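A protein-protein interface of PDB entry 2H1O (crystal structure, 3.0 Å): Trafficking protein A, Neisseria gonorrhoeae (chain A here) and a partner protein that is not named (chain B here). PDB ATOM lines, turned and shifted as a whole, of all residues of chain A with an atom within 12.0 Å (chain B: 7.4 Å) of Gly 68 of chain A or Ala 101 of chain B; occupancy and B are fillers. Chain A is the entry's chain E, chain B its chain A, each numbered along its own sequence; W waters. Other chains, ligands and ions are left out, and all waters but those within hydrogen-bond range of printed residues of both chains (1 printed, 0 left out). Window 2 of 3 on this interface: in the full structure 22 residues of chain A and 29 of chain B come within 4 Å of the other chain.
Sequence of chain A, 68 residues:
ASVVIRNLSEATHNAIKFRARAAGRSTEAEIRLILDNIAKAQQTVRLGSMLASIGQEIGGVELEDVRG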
ATOM      1  N   GLU A  64      24.594  27.305  -1.235  1.00  0.00           N
ATOM      2  CA  GLU A  64      23.351  28.055  -1.155  1.00  0.00           C
ATOM      3  C   GLU A  64      22.710  27.692   0.171  1.00  0.00           C
ATOM      4  O   GLU A  64      23.050  26.673   0.767  1.00  0.00           O
ATOM      5  CB  GLU A  64      22.421  27.686  -2.317  1.00  0.00           C
ATOM      6  CG  GLU A  64      21.063  28.385  -2.281  1.00  0.00           C
ATOM      7  CD  GLU A  64      20.207  28.076  -3.498  1.00  0.00           C
ATOM      8  OE1 GLU A  64      18.965  28.202  -3.401  1.00  0.00           O
ATOM      9  OE2 GLU A  64      20.775  27.717  -4.552  1.00  0.00           O
ATOM     10  N   ASP A  65      21.784  28.522   0.637  1.00  0.00           N
ATOM     11  CA  ASP A  65      21.136  28.255   1.911  1.00  0.00           C
ATOM     12  C   ASP A  65      20.254  27.017   1.859  1.00  0.00           C
ATOM     13  O   ASP A  65      20.564  25.996   2.489  1.00  0.00           O
ATOM     14  CB  ASP A  65      20.309  29.464   2.367  1.00  0.00           C
ATOM     15  CG  ASP A  65      19.930  29.393   3.856  1.00  0.00           C
ATOM     16  OD1 ASP A  65      19.123  28.512   4.241  1.00  0.00           O
ATOM     17  OD2 ASP A  65      20.450  30.217   4.642  1.00  0.00           O
ATOM     18  N   VAL A  66      19.157  27.110   1.115  1.00  0.00           N
ATOM     19  CA  VAL A  66      18.225  25.992   0.988  1.00  0.00           C
ATOM     20  C   VAL A  66      17.665  25.571   2.339  1.00  0.00           C
ATOM     21  O   VAL A  66      18.175  24.632   2.954  1.00  0.00           O
ATOM     22  CB  VAL A  66      18.899  24.745   0.384  1.00  0.00           C
ATOM     23  CG1 VAL A  66      17.836  23.679   0.094  1.00  0.00           C
ATOM     24  CG2 VAL A  66      19.683  25.124  -0.861  1.00  0.00           C
ATOM     25  N   ARG A  67      16.620  26.254   2.796  1.00  0.00           N
ATOM     26  CA  ARG A  67      15.999  25.934   4.075  1.00  0.00           C
ATOM     27  C   ARG A  67      14.956  26.994   4.372  1.00  0.00           C
ATOM     28  O   ARG A  67      15.292  28.151   4.640  1.00  0.00           O
ATOM     29  CB  ARG A  67      17.056  25.910   5.187  1.00  0.00           C
ATOM     30  CG  ARG A  67      16.636  25.238   6.495  1.00  0.00           C
ATOM     31  CD  ARG A  67      17.675  24.212   6.906  1.00  0.00           C
ATOM     32  NE  ARG A  67      17.606  23.855   8.319  1.00  0.00           N
ATOM     33  CZ  ARG A  67      18.430  22.993   8.909  1.00  0.00           C
ATOM     34  NH1 ARG A  67      19.386  22.390   8.211  1.00  0.00           N
ATOM     35  NH2 ARG A  67      18.309  22.742  10.204  1.00  0.00           N
ATOM     36  N   GLY A  68      13.691  26.585   4.317  1.00  0.00           N
ATOM     37  CA  GLY A  68      12.590  27.500   4.574  1.00  0.00           C
ATOM     38  C   GLY A  68      12.668  28.174   5.932  1.00  0.00           C
ATOM     39  O   GLY A  68      12.686  29.425   5.981  1.00  0.00           O
ATOM     40  OXT GLY A  68      12.712  27.445   6.947  1.00  0.00           O
ATOM     41  N   GLU B  42      21.002  18.191   2.646  1.00  0.00           N
ATOM     42  CA  GLU B  42      21.313  19.595   2.395  1.00  0.00           C
ATOM     43  C   GLU B  42      22.717  19.799   1.824  1.00  0.00           C
ATOM     44  O   GLU B  42      22.900  20.523   0.853  1.00  0.00           O
ATOM     45  CB  GLU B  42      21.156  20.402   3.683  1.00  0.00           C
ATOM     46  CG  GLU B  42      19.842  21.154   3.782  1.00  0.00           C
ATOM     47  CD  GLU B  42      19.603  21.755   5.163  1.00  0.00           C
ATOM     48  OE1 GLU B  42      20.500  22.448   5.707  1.00  0.00           O
ATOM     49  OE2 GLU B  42      18.500  21.537   5.708  1.00  0.00           O
ATOM     50  N   TYR B  86       8.963  15.030  16.548  1.00  0.00           N
ATOM     51  CA  TYR B  86       8.842  16.192  15.679  1.00  0.00           C
ATOM     52  C   TYR B  86       7.464  16.816  15.846  1.00  0.00           C
ATOM     53  O   TYR B  86       7.330  18.029  15.985  1.00  0.00           O
ATOM     54  CB  TYR B  86       9.028  15.761  14.229  1.00  0.00           C
ATOM     55  CG  TYR B  86       8.541  16.754  13.206  1.00  0.00           C
ATOM     56  CD1 TYR B  86       9.338  17.813  12.800  1.00  0.00           C
ATOM     57  CD2 TYR B  86       7.279  16.612  12.623  1.00  0.00           C
ATOM     58  CE1 TYR B  86       8.899  18.708  11.828  1.00  0.00           C
ATOM     59  CE2 TYR B  86       6.825  17.497  11.655  1.00  0.00           C
ATOM     60  CZ  TYR B  86       7.642  18.544  11.258  1.00  0.00           C
ATOM     61  OH  TYR B  86       7.209  19.416  10.281  1.00  0.00           O
ATOM     62  N   ARG B  90       7.158  20.856  17.431  1.00  0.00           N
ATOM     63  CA  ARG B  90       6.621  21.953  16.627  1.00  0.00           C
ATOM     64  C   ARG B  90       5.305  22.513  17.135  1.00  0.00           C
ATOM     65  O   ARG B  90       5.127  23.726  17.198  1.00  0.00           O
ATOM     66  CB  ARG B  90       6.440  21.529  15.163  1.00  0.00           C
ATOM     67  CG  ARG B  90       7.723  21.413  14.356  1.00  0.00           C
ATOM     68  CD  ARG B  90       7.440  21.475  12.858  1.00  0.00           C
ATOM     69  NE  ARG B  90       7.019  22.806  12.417  1.00  0.00           N
ATOM     70  CZ  ARG B  90       6.685  23.113  11.165  1.00  0.00           C
ATOM     71  NH1 ARG B  90       6.720  22.186  10.218  1.00  0.00           N
ATOM     72  NH2 ARG B  90       6.311  24.347  10.858  1.00  0.00           N
ATOM     73  N   LYS B  98       7.381  31.307  19.447  1.00  0.00           N
ATOM     74  CA  LYS B  98       8.343  31.036  18.374  1.00  0.00           C
ATOM     75  C   LYS B  98       7.993  29.786  17.570  1.00  0.00           C
ATOM     76  O   LYS B  98       8.041  28.675  18.090  1.00  0.00           O
ATOM     77  CB  LYS B  98       9.760  30.895  18.960  1.00  0.00           C
ATOM     78  CG  LYS B  98      10.938  31.209  18.002  1.00  0.00           C
ATOM     79  CD  LYS B  98      11.035  30.233  16.827  1.00  0.00           C
ATOM     80  CE  LYS B  98      12.464  30.135  16.250  1.00  0.00           C
ATOM     81  NZ  LYS B  98      13.028  31.383  15.637  1.00  0.00           N
ATOM     82  N   GLU B  99       7.642  29.972  16.302  1.00  0.00           N
ATOM     83  CA  GLU B  99       7.307  28.853  15.433  1.00  0.00           C
ATOM     84  C   GLU B  99       8.595  28.311  14.813  1.00  0.00           C
ATOM     85  O   GLU B  99       9.541  29.060  14.590  1.00  0.00           O
ATOM     86  CB  GLU B  99       6.336  29.310  14.346  1.00  0.00           C
ATOM     87  CG  GLU B  99       5.987  28.238  13.311  1.00  0.00           C
ATOM     88  CD  GLU B  99       4.844  28.659  12.385  1.00  0.00           C
ATOM     89  OE1 GLU B  99       4.692  28.053  11.296  1.00  0.00           O
ATOM     90  OE2 GLU B  99       4.091  29.591  12.753  1.00  0.00           O
ATOM     91  N   ILE B 100       8.627  27.012  14.535  1.00  0.00           N
ATOM     92  CA  ILE B 100       9.817  26.386  13.974  1.00  0.00           C
ATOM     93  C   ILE B 100       9.616  25.860  12.568  1.00  0.00           C
ATOM     94  O   ILE B 100       8.596  25.249  12.275  1.00  0.00           O
ATOM     95  CB  ILE B 100      10.246  25.222  14.835  1.00  0.00           C
ATOM     96  CG1 ILE B 100      10.296  25.662  16.292  1.00  0.00           C
ATOM     97  CG2 ILE B 100      11.589  24.736  14.393  1.00  0.00           C
ATOM     98  CD1 ILE B 100      10.509  24.528  17.265  1.00  0.00           C
ATOM     99  N   ALA B 101      10.602  26.081  11.704  1.00  0.00           N
ATOM    100  CA  ALA B 101      10.527  25.602  10.324  1.00  0.00           C
ATOM    101  C   ALA B 101      10.731  24.089  10.271  1.00  0.00           C
ATOM    102  O   ALA B 101      11.652  23.558  10.890  1.00  0.00           O
ATOM    103  CB  ALA B 101      11.574  26.286   9.479  1.00  0.00           C
ATOM    104  N   ALA B 102       9.884  23.398   9.519  1.00  0.00           N
ATOM    105  CA  ALA B 102       9.980  21.949   9.405  1.00  0.00           C
ATOM    106  C   ALA B 102      11.418  21.421   9.399  1.00  0.00           C
ATOM    107  O   ALA B 102      11.772  20.556  10.187  1.00  0.00           O
ATOM    108  CB  ALA B 102       9.252  21.490   8.159  1.00  0.00           C
ATOM    109  N   ALA B 103      12.248  21.935   8.506  1.00  0.00           N
ATOM    110  CA  ALA B 103      13.627  21.488   8.442  1.00  0.00           C
ATOM    111  C   ALA B 103      14.226  21.518   9.831  1.00  0.00           C
ATOM    112  O   ALA B 103      14.726  20.506  10.313  1.00  0.00           O
ATOM    113  CB  ALA B 103      14.423  22.378   7.520  1.00  0.00           C
ATOM    114  N   ASP B 104      14.167  22.676  10.482  1.00  0.00           N
ATOM    115  CA  ASP B 104      14.722  22.808  11.828  1.00  0.00           C
ATOM    116  C   ASP B 104      14.040  21.868  12.821  1.00  0.00           C
ATOM    117  O   ASP B 104      14.637  21.470  13.819  1.00  0.00           O
ATOM    118  CB  ASP B 104      14.605  24.250  12.331  1.00  0.00           C
ATOM    119  CG  ASP B 104      15.279  25.246  11.405  1.00  0.00           C
ATOM    120  OD1 ASP B 104      16.480  25.061  11.097  1.00  0.00           O
ATOM    121  OD2 ASP B 104      14.606  26.218  10.987  1.00  0.00           O
ATOM    122  N   GLY B 105      12.789  21.514  12.546  1.00  0.00           N
ATOM    123  CA  GLY B 105      12.081  20.615  13.432  1.00  0.00           C
ATOM    124  C   GLY B 105      12.610  19.201  13.285  1.00  0.00           C
ATOM    125  O   GLY B 105      12.673  18.446  14.253  1.00  0.00           O
ATOM    126  N   TYR B 106      12.990  18.841  12.066  1.00  0.00           N
ATOM    127  CA  TYR B 106      13.501  17.507  11.798  1.00  0.00           C
ATOM    128  C   TYR B 106      14.779  17.339  12.598  1.00  0.00           C
ATOM    129  O   TYR B 106      14.943  16.372  13.342  1.00  0.00           O
ATOM    130  CB  TYR B 106      13.763  17.324  10.284  1.00  0.00           C
ATOM    131  CG  TYR B 106      12.505  17.354   9.411  1.00  0.00           C
ATOM    132  CD1 TYR B 106      12.567  17.720   8.060  1.00  0.00           C
ATOM    133  CD2 TYR B 106      11.255  17.043   9.944  1.00  0.00           C
ATOM    134  CE1 TYR B 106      11.418  17.781   7.268  1.00  0.00           C
ATOM    135  CE2 TYR B 106      10.100  17.102   9.161  1.00  0.00           C
ATOM    136  CZ  TYR B 106      10.187  17.470   7.828  1.00  0.00           C
ATOM    137  OH  TYR B 106       9.031  17.520   7.078  1.00  0.00           O
ATOM    138  N   ILE B 107      15.673  18.309  12.461  1.00  0.00           N
ATOM    139  CA  ILE B 107      16.945  18.278  13.170  1.00  0.00           C
ATOM    140  C   ILE B 107      16.735  18.247  14.682  1.00  0.00           C
ATOM    141  O   ILE B 107      17.290  17.393  15.365  1.00  0.00           O
ATOM    142  CB  ILE B 107      17.840  19.504  12.773  1.00  0.00           C
ATOM    143  CG1 ILE B 107      18.600  19.217  11.467  1.00  0.00           C
ATOM    144  CG2 ILE B 107      18.843  19.800  13.873  1.00  0.00           C
ATOM    145  CD1 ILE B 107      17.718  19.007  10.251  1.00  0.00           C
ATOM    146  N   SER B 125      16.266  29.210  17.307  1.00  0.00           N
ATOM    147  CA  SER B 125      15.101  28.377  17.061  1.00  0.00           C
ATOM    148  C   SER B 125      15.058  27.170  17.991  1.00  0.00           C
ATOM    149  O   SER B 125      14.094  26.976  18.732  1.00  0.00           O
ATOM    150  CB  SER B 125      15.090  27.904  15.608  1.00  0.00           C
ATOM    151  OG  SER B 125      13.994  27.032  15.389  1.00  0.00           O
HETATM  152  O   HOH W   1      14.924  27.976   8.629  1.00  0.00           O
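Val 66 of chain A touches Glu 42 of chain B (O to CD, 3.9 Å).
Arg 67 of chain A touches Ala 103 of chain B.
Arg 67 of chain A touches Ile 107 of chain B (NH2 to CG1, 3.8 Å).
CB of Ala 101 of chain B touches OXT of Gly 68 of chain A, at 3.0 Å.
Water W1 bridges OXT of Gly 68 of chain A (2.8 Å) and OD2 of Asp 104 of chain B (3.0 Å).
Gly 68 of chain A touches just one residue of chain B: Ala 101.
Ala 101 of chain B touches one residue of chain A.
No residue of chain A comes within 4 Å of Glu 99 of chain B.
No residue of chain A comes within 4 Å of Ala 102 of chain B.
Of chain A, only Arg 67 (3.1 Å) comes within 4 Å of Asp 104 of chain B.
Printed residues of chain B within 4 Å of Arg 67 of chain A: Glu 42 (2.7 Å), Ala 103 (3.6 Å), Asp 104 (3.1 Å) and Ile 107 (3.8 Å).
Printed residues of chain A within 4 Å of Ile 107 of chain B: Arg 67 (3.8 Å).
Lys 98 of chain B touches none of the printed residues of chain A.
The nearest residue of chain B that does not touch Gly 68 of chain A is Asp 104 of chain B (4.6 Å).
OD1 of Asp 104 of chain B is in salt-bridge range of NH2 of Arg 67 of chain A, at 3.1 Å.
The side-chain carboxylate of Glu 42 of chain B is in salt-bridge range of the guanidinium group of Arg 67 of chain A, 2.7 Å away.
Of the 14 printed residues of chain B, 5 touch a printed residue of chain A.
Among the printed residues, Asp or Glu carboxylates within 4 Å of a Lys or Arg side-chain nitrogen of the other chain: Arg 67 of chain A with Glu 42 of chain B and Arg 67 of chain A with Asp 104 of chain B.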
